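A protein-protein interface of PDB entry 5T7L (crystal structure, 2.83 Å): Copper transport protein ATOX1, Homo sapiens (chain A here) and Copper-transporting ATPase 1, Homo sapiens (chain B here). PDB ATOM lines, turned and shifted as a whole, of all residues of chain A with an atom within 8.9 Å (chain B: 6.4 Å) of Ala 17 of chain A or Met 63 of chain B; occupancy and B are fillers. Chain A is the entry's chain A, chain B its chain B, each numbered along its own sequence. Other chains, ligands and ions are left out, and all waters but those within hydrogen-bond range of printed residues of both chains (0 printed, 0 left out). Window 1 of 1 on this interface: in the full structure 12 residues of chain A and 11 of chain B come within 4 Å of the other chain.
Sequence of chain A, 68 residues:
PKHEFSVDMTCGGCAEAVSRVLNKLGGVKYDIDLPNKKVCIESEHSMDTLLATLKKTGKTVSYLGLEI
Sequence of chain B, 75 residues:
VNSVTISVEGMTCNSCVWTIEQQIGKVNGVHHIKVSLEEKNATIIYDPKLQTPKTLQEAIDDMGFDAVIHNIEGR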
ATOM      1  N   VAL A   7       2.690 -15.376  19.076  1.00  0.00           N
ATOM      2  CA  VAL A   7       1.456 -16.148  19.226  1.00  0.00           C
ATOM      3  C   VAL A   7       0.279 -15.179  19.227  1.00  0.00           C
ATOM      4  O   VAL A   7       0.178 -14.334  20.124  1.00  0.00           O
ATOM      5  CB  VAL A   7       1.442 -16.989  20.515  1.00  0.00           C
ATOM      6  CG1 VAL A   7       0.284 -18.001  20.460  1.00  0.00           C
ATOM      7  CG2 VAL A   7       2.763 -17.687  20.729  1.00  0.00           C
ATOM      8  N   MET A   9      -2.784 -13.832  20.319  1.00  0.00           N
ATOM      9  CA  MET A   9      -3.484 -14.007  21.581  1.00  0.00           C
ATOM     10  C   MET A   9      -4.482 -12.870  21.711  1.00  0.00           C
ATOM     11  O   MET A   9      -4.095 -11.718  21.929  1.00  0.00           O
ATOM     12  CB  MET A   9      -2.508 -14.041  22.761  1.00  0.00           C
ATOM     13  CG  MET A   9      -1.671 -15.333  22.874  1.00  0.00           C
ATOM     14  SD  MET A   9      -0.586 -15.331  24.324  1.00  0.00           S
ATOM     15  CE  MET A   9       0.540 -13.983  23.940  1.00  0.00           C
ATOM     16  N   CYS A  11      -7.541 -12.780  23.811  1.00  0.00           N
ATOM     17  CA  CYS A  11      -8.129 -12.616  25.127  1.00  0.00           C
ATOM     18  C   CYS A  11      -7.139 -13.052  26.202  1.00  0.00           C
ATOM     19  O   CYS A  11      -6.059 -13.568  25.911  1.00  0.00           O
ATOM     20  CB  CYS A  11      -9.426 -13.425  25.208  1.00  0.00           C
ATOM     21  SG  CYS A  11     -10.139 -13.515  26.830  1.00  0.00           S
ATOM     22  N   GLY A  12      -7.506 -12.813  27.464  1.00  0.00           N
ATOM     23  CA  GLY A  12      -6.710 -13.332  28.562  1.00  0.00           C
ATOM     24  C   GLY A  12      -6.814 -14.836  28.683  1.00  0.00           C
ATOM     25  O   GLY A  12      -5.853 -15.500  29.082  1.00  0.00           O
ATOM     26  N   GLY A  13      -7.971 -15.396  28.332  1.00  0.00           N
ATOM     27  CA  GLY A  13      -8.094 -16.839  28.280  1.00  0.00           C
ATOM     28  C   GLY A  13      -7.196 -17.471  27.241  1.00  0.00           C
ATOM     29  O   GLY A  13      -6.716 -18.595  27.428  1.00  0.00           O
ATOM     30  N   CYS A  14      -6.966 -16.771  26.124  1.00  0.00           N
ATOM     31  CA  CYS A  14      -6.030 -17.253  25.116  1.00  0.00           C
ATOM     32  C   CYS A  14      -4.628 -17.384  25.699  1.00  0.00           C
ATOM     33  O   CYS A  14      -3.901 -18.333  25.379  1.00  0.00           O
ATOM     34  CB  CYS A  14      -6.027 -16.314  23.905  1.00  0.00           C
ATOM     35  SG  CYS A  14      -7.512 -16.355  22.857  1.00  0.00           S
ATOM     36  N   ALA A  15      -4.236 -16.446  26.567  1.00  0.00           N
ATOM     37  CA  ALA A  15      -2.906 -16.483  27.163  1.00  0.00           C
ATOM     38  C   ALA A  15      -2.808 -17.556  28.227  1.00  0.00           C
ATOM     39  O   ALA A  15      -1.725 -18.106  28.450  1.00  0.00           O
ATOM     40  CB  ALA A  15      -2.543 -15.125  27.764  1.00  0.00           C
ATOM     41  N   GLU A  16      -3.915 -17.859  28.904  1.00  0.00           N
ATOM     42  CA  GLU A  16      -3.897 -18.951  29.866  1.00  0.00           C
ATOM     43  C   GLU A  16      -3.688 -20.292  29.190  1.00  0.00           C
ATOM     44  O   GLU A  16      -3.110 -21.202  29.789  1.00  0.00           O
ATOM     45  CB  GLU A  16      -5.188 -18.991  30.659  1.00  0.00           C
ATOM     46  CG  GLU A  16      -5.264 -17.957  31.719  1.00  0.00           C
ATOM     47  CD  GLU A  16      -6.683 -17.731  32.143  1.00  0.00           C
ATOM     48  OE1 GLU A  16      -7.511 -18.657  31.961  1.00  0.00           O
ATOM     49  OE2 GLU A  16      -6.971 -16.634  32.658  1.00  0.00           O
ATOM     50  N   ALA A  17      -4.163 -20.452  27.955  1.00  0.00           N
ATOM     51  CA  ALA A  17      -3.922 -21.721  27.284  1.00  0.00           C
ATOM     52  C   ALA A  17      -2.444 -21.879  26.915  1.00  0.00           C
ATOM     53  O   ALA A  17      -1.906 -22.987  26.999  1.00  0.00           O
ATOM     54  CB  ALA A  17      -4.836 -21.863  26.062  1.00  0.00           C
ATOM     55  N   VAL A  18      -1.762 -20.785  26.558  1.00  0.00           N
ATOM     56  CA  VAL A  18      -0.358 -20.886  26.167  1.00  0.00           C
ATOM     57  C   VAL A  18       0.492 -21.386  27.332  1.00  0.00           C
ATOM     58  O   VAL A  18       1.352 -22.259  27.161  1.00  0.00           O
ATOM     59  CB  VAL A  18       0.139 -19.532  25.624  1.00  0.00           C
ATOM     60  CG1 VAL A  18       1.670 -19.471  25.588  1.00  0.00           C
ATOM     61  CG2 VAL A  18      -0.402 -19.313  24.244  1.00  0.00           C
ATOM     62  N   SER A  19       0.249 -20.865  28.537  1.00  0.00           N
ATOM     63  CA  SER A  19       0.997 -21.261  29.728  1.00  0.00           C
ATOM     64  C   SER A  19       0.686 -22.674  30.193  1.00  0.00           C
ATOM     65  O   SER A  19       1.349 -23.169  31.109  1.00  0.00           O
ATOM     66  CB  SER A  19       0.704 -20.301  30.872  1.00  0.00           C
ATOM     67  OG  SER A  19      -0.601 -20.532  31.356  1.00  0.00           O
ATOM     68  N   ARG A  20      -0.316 -23.325  29.614  1.00  0.00           N
ATOM     69  CA  ARG A  20      -0.702 -24.672  30.000  1.00  0.00           C
ATOM     70  C   ARG A  20      -0.019 -25.725  29.146  1.00  0.00           C
ATOM     71  O   ARG A  20       0.601 -26.655  29.672  1.00  0.00           O
ATOM     72  CB  ARG A  20      -2.213 -24.807  29.901  1.00  0.00           C
ATOM     73  CG  ARG A  20      -2.904 -24.042  30.987  1.00  0.00           C
ATOM     74  CD  ARG A  20      -3.234 -24.996  32.083  1.00  0.00           C
ATOM     75  NE  ARG A  20      -3.925 -26.141  31.517  1.00  0.00           N
ATOM     76  CZ  ARG A  20      -3.740 -27.392  31.909  1.00  0.00           C
ATOM     77  NH1 ARG A  20      -2.863 -27.666  32.867  1.00  0.00           N
ATOM     78  NH2 ARG A  20      -4.424 -28.368  31.326  1.00  0.00           N
ATOM     79  N   VAL A  21      -0.120 -25.583  27.827  1.00  0.00           N
ATOM     80  CA  VAL A  21       0.671 -26.415  26.942  1.00  0.00           C
ATOM     81  C   VAL A  21       2.148 -26.306  27.279  1.00  0.00           C
ATOM     82  O   VAL A  21       2.886 -27.289  27.153  1.00  0.00           O
ATOM     83  CB  VAL A  21       0.369 -26.049  25.476  1.00  0.00           C
ATOM     84  CG1 VAL A  21      -1.126 -26.125  25.244  1.00  0.00           C
ATOM     85  CG2 VAL A  21       0.918 -24.677  25.115  1.00  0.00           C
ATOM     86  N   LEU A  22       2.602 -25.127  27.730  1.00  0.00           N
ATOM     87  CA  LEU A  22       3.997 -24.956  28.143  1.00  0.00           C
ATOM     88  C   LEU A  22       4.275 -25.696  29.448  1.00  0.00           C
ATOM     89  O   LEU A  22       5.265 -26.432  29.556  1.00  0.00           O
ATOM     90  CB  LEU A  22       4.335 -23.469  28.287  1.00  0.00           C
ATOM     91  CG  LEU A  22       4.614 -22.680  27.002  1.00  0.00           C
ATOM     92  CD1 LEU A  22       4.831 -21.226  27.330  1.00  0.00           C
ATOM     93  CD2 LEU A  22       5.820 -23.211  26.262  1.00  0.00           C
ATOM     94  N   ASN A  23       3.397 -25.524  30.444  1.00  0.00           N
ATOM     95  CA  ASN A  23       3.561 -26.193  31.734  1.00  0.00           C
ATOM     96  C   ASN A  23       3.489 -27.725  31.615  1.00  0.00           C
ATOM     97  O   ASN A  23       4.058 -28.438  32.448  1.00  0.00           O
ATOM     98  CB  ASN A  23       2.506 -25.663  32.710  1.00  0.00           C
ATOM     99  CG  ASN A  23       2.525 -26.372  34.066  1.00  0.00           C
ATOM    100  OD1 ASN A  23       3.493 -26.267  34.822  1.00  0.00           O
ATOM    101  ND2 ASN A  23       1.445 -27.098  34.379  1.00  0.00           N
ATOM    102  N   LYS A  24       2.814 -28.253  30.596  1.00  0.00           N
ATOM    103  CA  LYS A  24       2.726 -29.700  30.446  1.00  0.00           C
ATOM    104  C   LYS A  24       3.894 -30.280  29.667  1.00  0.00           C
ATOM    105  O   LYS A  24       4.253 -31.444  29.876  1.00  0.00           O
ATOM    106  CB  LYS A  24       1.414 -30.092  29.762  1.00  0.00           C
ATOM    107  CG  LYS A  24       0.181 -29.812  30.613  1.00  0.00           C
ATOM    108  CD  LYS A  24      -1.059 -30.440  30.007  1.00  0.00           C
ATOM    109  CE  LYS A  24      -2.006 -29.388  29.493  1.00  0.00           C
ATOM    110  NZ  LYS A  24      -3.301 -29.977  29.070  1.00  0.00           N
ATOM    111  N   TYR A  30       8.816 -19.567  31.288  1.00  0.00           N
ATOM    112  CA  TYR A  30       8.274 -18.698  30.249  1.00  0.00           C
ATOM    113  C   TYR A  30       7.730 -17.384  30.822  1.00  0.00           C
ATOM    114  O   TYR A  30       7.459 -17.249  32.024  1.00  0.00           O
ATOM    115  CB  TYR A  30       7.158 -19.422  29.472  1.00  0.00           C
ATOM    116  CG  TYR A  30       6.089 -19.941  30.393  1.00  0.00           C
ATOM    117  CD1 TYR A  30       5.085 -19.108  30.854  1.00  0.00           C
ATOM    118  CD2 TYR A  30       6.105 -21.250  30.838  1.00  0.00           C
ATOM    119  CE1 TYR A  30       4.125 -19.566  31.714  1.00  0.00           C
ATOM    120  CE2 TYR A  30       5.144 -21.714  31.704  1.00  0.00           C
ATOM    121  CZ  TYR A  30       4.157 -20.865  32.138  1.00  0.00           C
ATOM    122  OH  TYR A  30       3.190 -21.308  33.000  1.00  0.00           O
ATOM    123  N   ILE A  32       4.705 -14.613  29.236  1.00  0.00           N
ATOM    124  CA  ILE A  32       3.732 -14.401  28.156  1.00  0.00           C
ATOM    125  C   ILE A  32       3.237 -12.960  28.220  1.00  0.00           C
ATOM    126  O   ILE A  32       2.560 -12.576  29.180  1.00  0.00           O
ATOM    127  CB  ILE A  32       2.553 -15.387  28.252  1.00  0.00           C
ATOM    128  CG1 ILE A  32       3.056 -16.812  28.393  1.00  0.00           C
ATOM    129  CG2 ILE A  32       1.678 -15.342  27.011  1.00  0.00           C
ATOM    130  CD1 ILE A  32       1.996 -17.742  28.779  1.00  0.00           C
ATOM    131  N   VAL A  39       5.662 -14.645  23.129  1.00  0.00           N
ATOM    132  CA  VAL A  39       6.118 -15.578  24.155  1.00  0.00           C
ATOM    133  C   VAL A  39       7.636 -15.675  24.072  1.00  0.00           C
ATOM    134  O   VAL A  39       8.199 -15.746  22.975  1.00  0.00           O
ATOM    135  CB  VAL A  39       5.463 -16.973  23.999  1.00  0.00           C
ATOM    136  CG1 VAL A  39       5.851 -17.870  25.156  1.00  0.00           C
ATOM    137  CG2 VAL A  39       3.952 -16.835  23.929  1.00  0.00           C
ATOM    138  N   THR A  53       4.802 -27.335  20.570  1.00  0.00           N
ATOM    139  CA  THR A  53       3.951 -27.234  21.750  1.00  0.00           C
ATOM    140  C   THR A  53       2.970 -26.076  21.613  1.00  0.00           C
ATOM    141  O   THR A  53       1.768 -26.233  21.860  1.00  0.00           O
ATOM    142  CB  THR A  53       4.798 -27.066  23.016  1.00  0.00           C
ATOM    143  OG1 THR A  53       5.637 -28.212  23.188  1.00  0.00           O
ATOM    144  CG2 THR A  53       3.898 -26.893  24.264  1.00  0.00           C
ATOM    145  N   LEU A  54       3.458 -24.908  21.191  1.00  0.00           N
ATOM    146  CA  LEU A  54       2.608 -23.733  21.189  1.00  0.00           C
ATOM    147  C   LEU A  54       1.516 -23.771  20.116  1.00  0.00           C
ATOM    148  O   LEU A  54       0.502 -23.083  20.291  1.00  0.00           O
ATOM    149  CB  LEU A  54       3.462 -22.472  21.057  1.00  0.00           C
ATOM    150  CG  LEU A  54       4.452 -22.103  22.186  1.00  0.00           C
ATOM    151  CD1 LEU A  54       5.670 -21.382  21.593  1.00  0.00           C
ATOM    152  CD2 LEU A  54       3.852 -21.260  23.334  1.00  0.00           C
ATOM    153  N   LYS A  55       1.642 -24.546  19.019  1.00  0.00           N
ATOM    154  CA  LYS A  55       0.462 -24.514  18.142  1.00  0.00           C
ATOM    155  C   LYS A  55      -0.602 -25.535  18.518  1.00  0.00           C
ATOM    156  O   LYS A  55      -1.633 -25.620  17.837  1.00  0.00           O
ATOM    157  CB  LYS A  55       0.738 -24.717  16.645  1.00  0.00           C
ATOM    158  CG  LYS A  55       1.962 -24.155  16.035  1.00  0.00           C
ATOM    159  CD  LYS A  55       2.963 -25.225  16.131  1.00  0.00           C
ATOM    160  CE  LYS A  55       4.122 -24.984  15.220  1.00  0.00           C
ATOM    161  NZ  LYS A  55       5.106 -26.090  15.370  1.00  0.00           N
ATOM    162  N   LYS A  56      -0.406 -26.303  19.575  1.00  0.00           N
ATOM    163  CA  LYS A  56      -1.529 -27.093  20.043  1.00  0.00           C
ATOM    164  C   LYS A  56      -2.666 -26.219  20.552  1.00  0.00           C
ATOM    165  O   LYS A  56      -3.768 -26.734  20.766  1.00  0.00           O
ATOM    166  CB  LYS A  56      -1.048 -28.062  21.122  1.00  0.00           C
ATOM    167  CG  LYS A  56      -0.046 -29.069  20.598  1.00  0.00           C
ATOM    168  CD  LYS A  56       0.534 -29.882  21.721  1.00  0.00           C
ATOM    169  CE  LYS A  56       1.374 -31.028  21.169  1.00  0.00           C
ATOM    170  NZ  LYS A  56       1.850 -31.951  22.237  1.00  0.00           N
ATOM    171  N   THR A  57      -2.425 -24.910  20.729  1.00  0.00           N
ATOM    172  CA  THR A  57      -3.455 -23.970  21.160  1.00  0.00           C
ATOM    173  C   THR A  57      -4.537 -23.789  20.106  1.00  0.00           C
ATOM    174  O   THR A  57      -5.633 -23.316  20.435  1.00  0.00           O
ATOM    175  CB  THR A  57      -2.850 -22.586  21.481  1.00  0.00           C
ATOM    176  OG1 THR A  57      -2.157 -22.089  20.337  1.00  0.00           O
ATOM    177  CG2 THR A  57      -1.887 -22.605  22.671  1.00  0.00           C
ATOM    178  N   GLY A  58      -4.258 -24.159  18.853  1.00  0.00           N
ATOM    179  CA  GLY A  58      -5.067 -23.749  17.727  1.00  0.00           C
ATOM    180  C   GLY A  58      -4.666 -22.413  17.137  1.00  0.00           C
ATOM    181  O   GLY A  58      -5.111 -22.077  16.029  1.00  0.00           O
ATOM    182  N   LYS A  59      -3.825 -21.652  17.838  1.00  0.00           N
ATOM    183  CA  LYS A  59      -3.411 -20.316  17.434  1.00  0.00           C
ATOM    184  C   LYS A  59      -2.203 -20.379  16.492  1.00  0.00           C
ATOM    185  O   LYS A  59      -1.333 -21.250  16.625  1.00  0.00           O
ATOM    186  CB  LYS A  59      -3.095 -19.498  18.684  1.00  0.00           C
ATOM    187  CG  LYS A  59      -4.282 -19.403  19.636  1.00  0.00           C
ATOM    188  CD  LYS A  59      -5.415 -18.609  18.966  1.00  0.00           C
ATOM    189  CE  LYS A  59      -6.566 -18.265  19.905  1.00  0.00           C
ATOM    190  NZ  LYS A  59      -7.298 -17.039  19.444  1.00  0.00           N
ATOM    191  N   GLY B  10     -11.451 -22.311  31.940  1.00  0.00           N
ATOM    192  CA  GLY B  10     -10.537 -21.422  31.268  1.00  0.00           C
ATOM    193  C   GLY B  10     -11.046 -20.787  29.998  1.00  0.00           C
ATOM    194  O   GLY B  10     -10.267 -20.112  29.307  1.00  0.00           O
ATOM    195  N   THR B  19     -12.133 -20.805  19.063  1.00  0.00           N
ATOM    196  CA  THR B  19     -10.924 -21.600  18.892  1.00  0.00           C
ATOM    197  C   THR B  19     -11.269 -23.060  19.119  1.00  0.00           C
ATOM    198  O   THR B  19     -11.073 -23.904  18.244  1.00  0.00           O
ATOM    199  CB  THR B  19      -9.822 -21.177  19.879  1.00  0.00           C
ATOM    200  OG1 THR B  19      -9.839 -19.753  20.036  1.00  0.00           O
ATOM    201  CG2 THR B  19      -8.456 -21.610  19.370  1.00  0.00           C
ATOM    202  N   ILE B  20     -11.789 -23.349  20.306  1.00  0.00           N
ATOM    203  CA  ILE B  20     -12.193 -24.706  20.649  1.00  0.00           C
ATOM    204  C   ILE B  20     -13.181 -25.237  19.618  1.00  0.00           C
ATOM    205  O   ILE B  20     -13.036 -26.354  19.109  1.00  0.00           O
ATOM    206  CB  ILE B  20     -12.783 -24.763  22.071  1.00  0.00           C
ATOM    207  CG1 ILE B  20     -11.753 -24.276  23.114  1.00  0.00           C
ATOM    208  CG2 ILE B  20     -13.280 -26.182  22.353  1.00  0.00           C
ATOM    209  CD1 ILE B  20     -12.255 -24.289  24.587  1.00  0.00           C
ATOM    210  N   GLU B  21     -14.194 -24.433  19.282  1.00  0.00           N
ATOM    211  CA  GLU B  21     -15.219 -24.894  18.351  1.00  0.00           C
ATOM    212  C   GLU B  21     -14.644 -25.168  16.973  1.00  0.00           C
ATOM    213  O   GLU B  21     -14.966 -26.180  16.345  1.00  0.00           O
ATOM    214  CB  GLU B  21     -16.336 -23.867  18.246  1.00  0.00           C
ATOM    215  CG  GLU B  21     -17.650 -24.332  18.795  1.00  0.00           C
ATOM    216  CD  GLU B  21     -18.575 -23.178  19.076  1.00  0.00           C
ATOM    217  OE1 GLU B  21     -18.312 -22.073  18.556  1.00  0.00           O
ATOM    218  OE2 GLU B  21     -19.551 -23.367  19.831  1.00  0.00           O
ATOM    219  N   GLN B  23     -11.746 -25.947  15.789  1.00  0.00           N
ATOM    220  CA  GLN B  23     -10.733 -26.953  15.532  1.00  0.00           C
ATOM    221  C   GLN B  23     -11.175 -28.344  15.946  1.00  0.00           C
ATOM    222  O   GLN B  23     -10.876 -29.312  15.249  1.00  0.00           O
ATOM    223  CB  GLN B  23      -9.426 -26.562  16.229  1.00  0.00           C
ATOM    224  CG  GLN B  23      -8.475 -27.692  16.525  1.00  0.00           C
ATOM    225  CD  GLN B  23      -7.058 -27.185  16.657  1.00  0.00           C
ATOM    226  OE1 GLN B  23      -6.742 -26.106  16.156  1.00  0.00           O
ATOM    227  NE2 GLN B  23      -6.197 -27.953  17.321  1.00  0.00           N
ATOM    228  N   ILE B  24     -11.923 -28.462  17.043  1.00  0.00           N
ATOM    229  CA  ILE B  24     -12.545 -29.733  17.380  1.00  0.00           C
ATOM    230  C   ILE B  24     -13.617 -30.099  16.355  1.00  0.00           C
ATOM    231  O   ILE B  24     -13.997 -31.272  16.244  1.00  0.00           O
ATOM    232  CB  ILE B  24     -13.091 -29.656  18.820  1.00  0.00           C
ATOM    233  CG1 ILE B  24     -11.955 -29.303  19.781  1.00  0.00           C
ATOM    234  CG2 ILE B  24     -13.751 -30.959  19.254  1.00  0.00           C
ATOM    235  CD1 ILE B  24     -10.956 -30.397  20.000  1.00  0.00           C
ATOM    236  N   GLU B  58      -9.413 -35.531  25.534  1.00  0.00           N
ATOM    237  CA  GLU B  58      -7.980 -35.285  25.392  1.00  0.00           C
ATOM    238  C   GLU B  58      -7.682 -34.225  24.327  1.00  0.00           C
ATOM    239  O   GLU B  58      -6.792 -33.388  24.524  1.00  0.00           O
ATOM    240  CB  GLU B  58      -7.271 -36.607  25.079  1.00  0.00           C
ATOM    241  CG  GLU B  58      -5.864 -36.756  25.680  1.00  0.00           C
ATOM    242  CD  GLU B  58      -5.189 -38.084  25.311  1.00  0.00           C
ATOM    243  OE1 GLU B  58      -5.853 -39.140  25.428  1.00  0.00           O
ATOM    244  OE2 GLU B  58      -3.997 -38.065  24.909  1.00  0.00           O
ATOM    245  N   ALA B  59      -8.424 -34.227  23.212  1.00  0.00           N
ATOM    246  CA  ALA B  59      -8.245 -33.204  22.178  1.00  0.00           C
ATOM    247  C   ALA B  59      -8.383 -31.792  22.747  1.00  0.00           C
ATOM    248  O   ALA B  59      -7.575 -30.901  22.442  1.00  0.00           O
ATOM    249  CB  ALA B  59      -9.256 -33.416  21.051  1.00  0.00           C
ATOM    250  N   ILE B  60      -9.423 -31.568  23.560  1.00  0.00           N
ATOM    251  CA  ILE B  60      -9.604 -30.271  24.200  1.00  0.00           C
ATOM    252  C   ILE B  60      -8.482 -30.010  25.196  1.00  0.00           C
ATOM    253  O   ILE B  60      -7.862 -28.946  25.179  1.00  0.00           O
ATOM    254  CB  ILE B  60     -10.990 -30.192  24.868  1.00  0.00           C
ATOM    255  CG1 ILE B  60     -12.080 -30.384  23.821  1.00  0.00           C
ATOM    256  CG2 ILE B  60     -11.188 -28.837  25.612  1.00  0.00           C
ATOM    257  CD1 ILE B  60     -13.450 -30.473  24.421  1.00  0.00           C
ATOM    258  N   ASP B  61      -8.209 -30.979  26.077  1.00  0.00           N
ATOM    259  CA  ASP B  61      -7.133 -30.839  27.065  1.00  0.00           C
ATOM    260  C   ASP B  61      -5.804 -30.415  26.417  1.00  0.00           C
ATOM    261  O   ASP B  61      -5.092 -29.550  26.950  1.00  0.00           O
ATOM    262  CB  ASP B  61      -6.984 -32.167  27.829  1.00  0.00           C
ATOM    263  CG  ASP B  61      -6.460 -31.998  29.256  1.00  0.00           C
ATOM    264  OD1 ASP B  61      -5.311 -32.420  29.513  1.00  0.00           O
ATOM    265  OD2 ASP B  61      -7.198 -31.490  30.129  1.00  0.00           O
ATOM    266  N   ASP B  62      -5.458 -30.996  25.257  1.00  0.00           N
ATOM    267  CA  ASP B  62      -4.200 -30.653  24.591  1.00  0.00           C
ATOM    268  C   ASP B  62      -4.157 -29.220  24.066  1.00  0.00           C
ATOM    269  O   ASP B  62      -3.083 -28.767  23.656  1.00  0.00           O
ATOM    270  CB  ASP B  62      -3.883 -31.638  23.438  1.00  0.00           C
ATOM    271  CG  ASP B  62      -3.363 -33.005  23.936  1.00  0.00           C
ATOM    272  OD1 ASP B  62      -2.175 -33.314  23.664  1.00  0.00           O
ATOM    273  OD2 ASP B  62      -4.119 -33.774  24.571  1.00  0.00           O
ATOM    274  N   MET B  63      -5.280 -28.501  24.059  1.00  0.00           N
ATOM    275  CA  MET B  63      -5.317 -27.115  23.608  1.00  0.00           C
ATOM    276  C   MET B  63      -4.973 -26.120  24.703  1.00  0.00           C
ATOM    277  O   MET B  63      -4.820 -24.929  24.407  1.00  0.00           O
ATOM    278  CB  MET B  63      -6.699 -26.769  23.062  1.00  0.00           C
ATOM    279  CG  MET B  63      -7.077 -27.510  21.825  1.00  0.00           C
ATOM    280  SD  MET B  63      -8.565 -26.812  21.081  1.00  0.00           S
ATOM    281  CE  MET B  63      -7.895 -25.409  20.220  1.00  0.00           C
ATOM    282  N   GLY B  64      -4.860 -26.568  25.947  1.00  0.00           N
ATOM    283  CA  GLY B  64      -4.573 -25.701  27.069  1.00  0.00           C
ATOM    284  C   GLY B  64      -5.776 -25.330  27.899  1.00  0.00           C
ATOM    285  O   GLY B  64      -5.657 -24.487  28.794  1.00  0.00           O
ATOM    286  N   PHE B  65      -6.938 -25.892  27.601  1.00  0.00           N
ATOM    287  CA  PHE B  65      -8.108 -25.760  28.446  1.00  0.00           C
ATOM    288  C   PHE B  65      -8.249 -27.060  29.205  1.00  0.00           C
ATOM    289  O   PHE B  65      -7.954 -28.123  28.662  1.00  0.00           O
ATOM    290  CB  PHE B  65      -9.347 -25.455  27.607  1.00  0.00           C
ATOM    291  CG  PHE B  65      -9.142 -24.322  26.648  1.00  0.00           C
ATOM    292  CD1 PHE B  65      -9.269 -23.007  27.071  1.00  0.00           C
ATOM    293  CD2 PHE B  65      -8.774 -24.567  25.337  1.00  0.00           C
ATOM    294  CE1 PHE B  65      -9.057 -21.968  26.195  1.00  0.00           C
ATOM    295  CE2 PHE B  65      -8.567 -23.538  24.462  1.00  0.00           C
ATOM    296  CZ  PHE B  65      -8.711 -22.234  24.889  1.00  0.00           C
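Of the 26 printed residues of chain A, 8 touch a printed residue of chain B. Hydrophobic or aromatic side chains of chain A that line the printed part of chain B: Ala 17 and Val 21. Of the 14 printed residues of chain B, 6 touch a printed residue of chain A. Printed residues of chain B that touch a printed residue of chain A: Thr 19, Gln 23, Asp 61, Asp 62, Met 63 and Gly 64. Hydrophobic or aromatic side chains of chain B within 4 Å of the printed part of chain A: Met 63. Among the printed residues, 13 pairs touch across the chains. Among the printed residues, Asp or Glu carboxylates within 4 Å of a Lys or Arg side-chain nitrogen of the other chain: Lys 24 of chain A with Asp 61 of chain B (3.2 Å).
Among the printed residues, pairs that only touch across the chains: Ala 17 of chain A with Met 63 of chain B (3.5 Å), Ala 17 of chain A with Gly 64 of chain B (3.6 Å), Arg 20 of chain A with Gly 64 of chain B (3.5 Å), Val 21 of chain A with Asp 62 of chain B (3.7 Å), Val 21 of chain A with Met 63 of chain B (3.9 Å), Val 21 of chain A with Gly 64 of chain B (3.8 Å), Lys 56 of chain A with Asp 62 of chain B (3.3 Å), Lys 56 of chain A with Met 63 of chain B (3.3 Å), Thr 57 of chain A with Thr 19 of chain B (3.5 Å), Thr 57 of chain A with Met 63 of chain B (3.1 Å), Gly 58 of chain A with Gln 23 of chain B (3.3 Å) and Lys 59 of chain A with Thr 19 of chain B (3.6 Å).
The side-chain amino group of Lys 59 of chain A sits close to the side-chain sulfur of Cys 14 of chain A (3.5 Å). O of Leu 54 of chain A lies within hydrogen-bond range of OG1 of Thr 57 of chain A (2.8 Å). The side-chain hydroxyl (OG1) of Thr 57 of chain A sits at hydrogen-bond distance from the backbone NH (N) of Lys 59 of chain A, at 3.0 Å. The side-chain carboxylate (OD2) of Asp 62 of chain B sits close to the backbone carbonyl oxygen (O) of Glu 58 of chain B (2.7 Å).
The side-chain amino group (NZ) of Lys 24 of chain A is in salt-bridge range of the side-chain carboxylate (OD1) of Asp 61 of chain B, at 3.2 Å.
Ala 17 of chain A touches just these residues of chain B: Met 63 and Gly 64. Ser 19 of chain A touches none of the printed residues of chain B. Printed residues of chain B within 4 Å of Lys 24 of chain A: Asp 61 (2.8 Å). Printed residues of chain B within 4 Å of Gly 58 of chain A: Gln 23 (3.3 Å). Of the printed residues of chain B, Lys 59 of chain A touches Thr 19. Printed residues of chain A within 4 Å of Thr 19 of chain B: Thr 57 and Lys 59. Of the printed residues of chain A, Asp 62 of chain B touches Val 21 and Lys 56. Of the printed residues of chain A, Met 63 of chain B touches Ala 17, Val 21, Lys 56 and Thr 57. The nearest residue of chain A that does not touch Met 63 of chain B is Gly 58 of chain A (4.1 Å).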
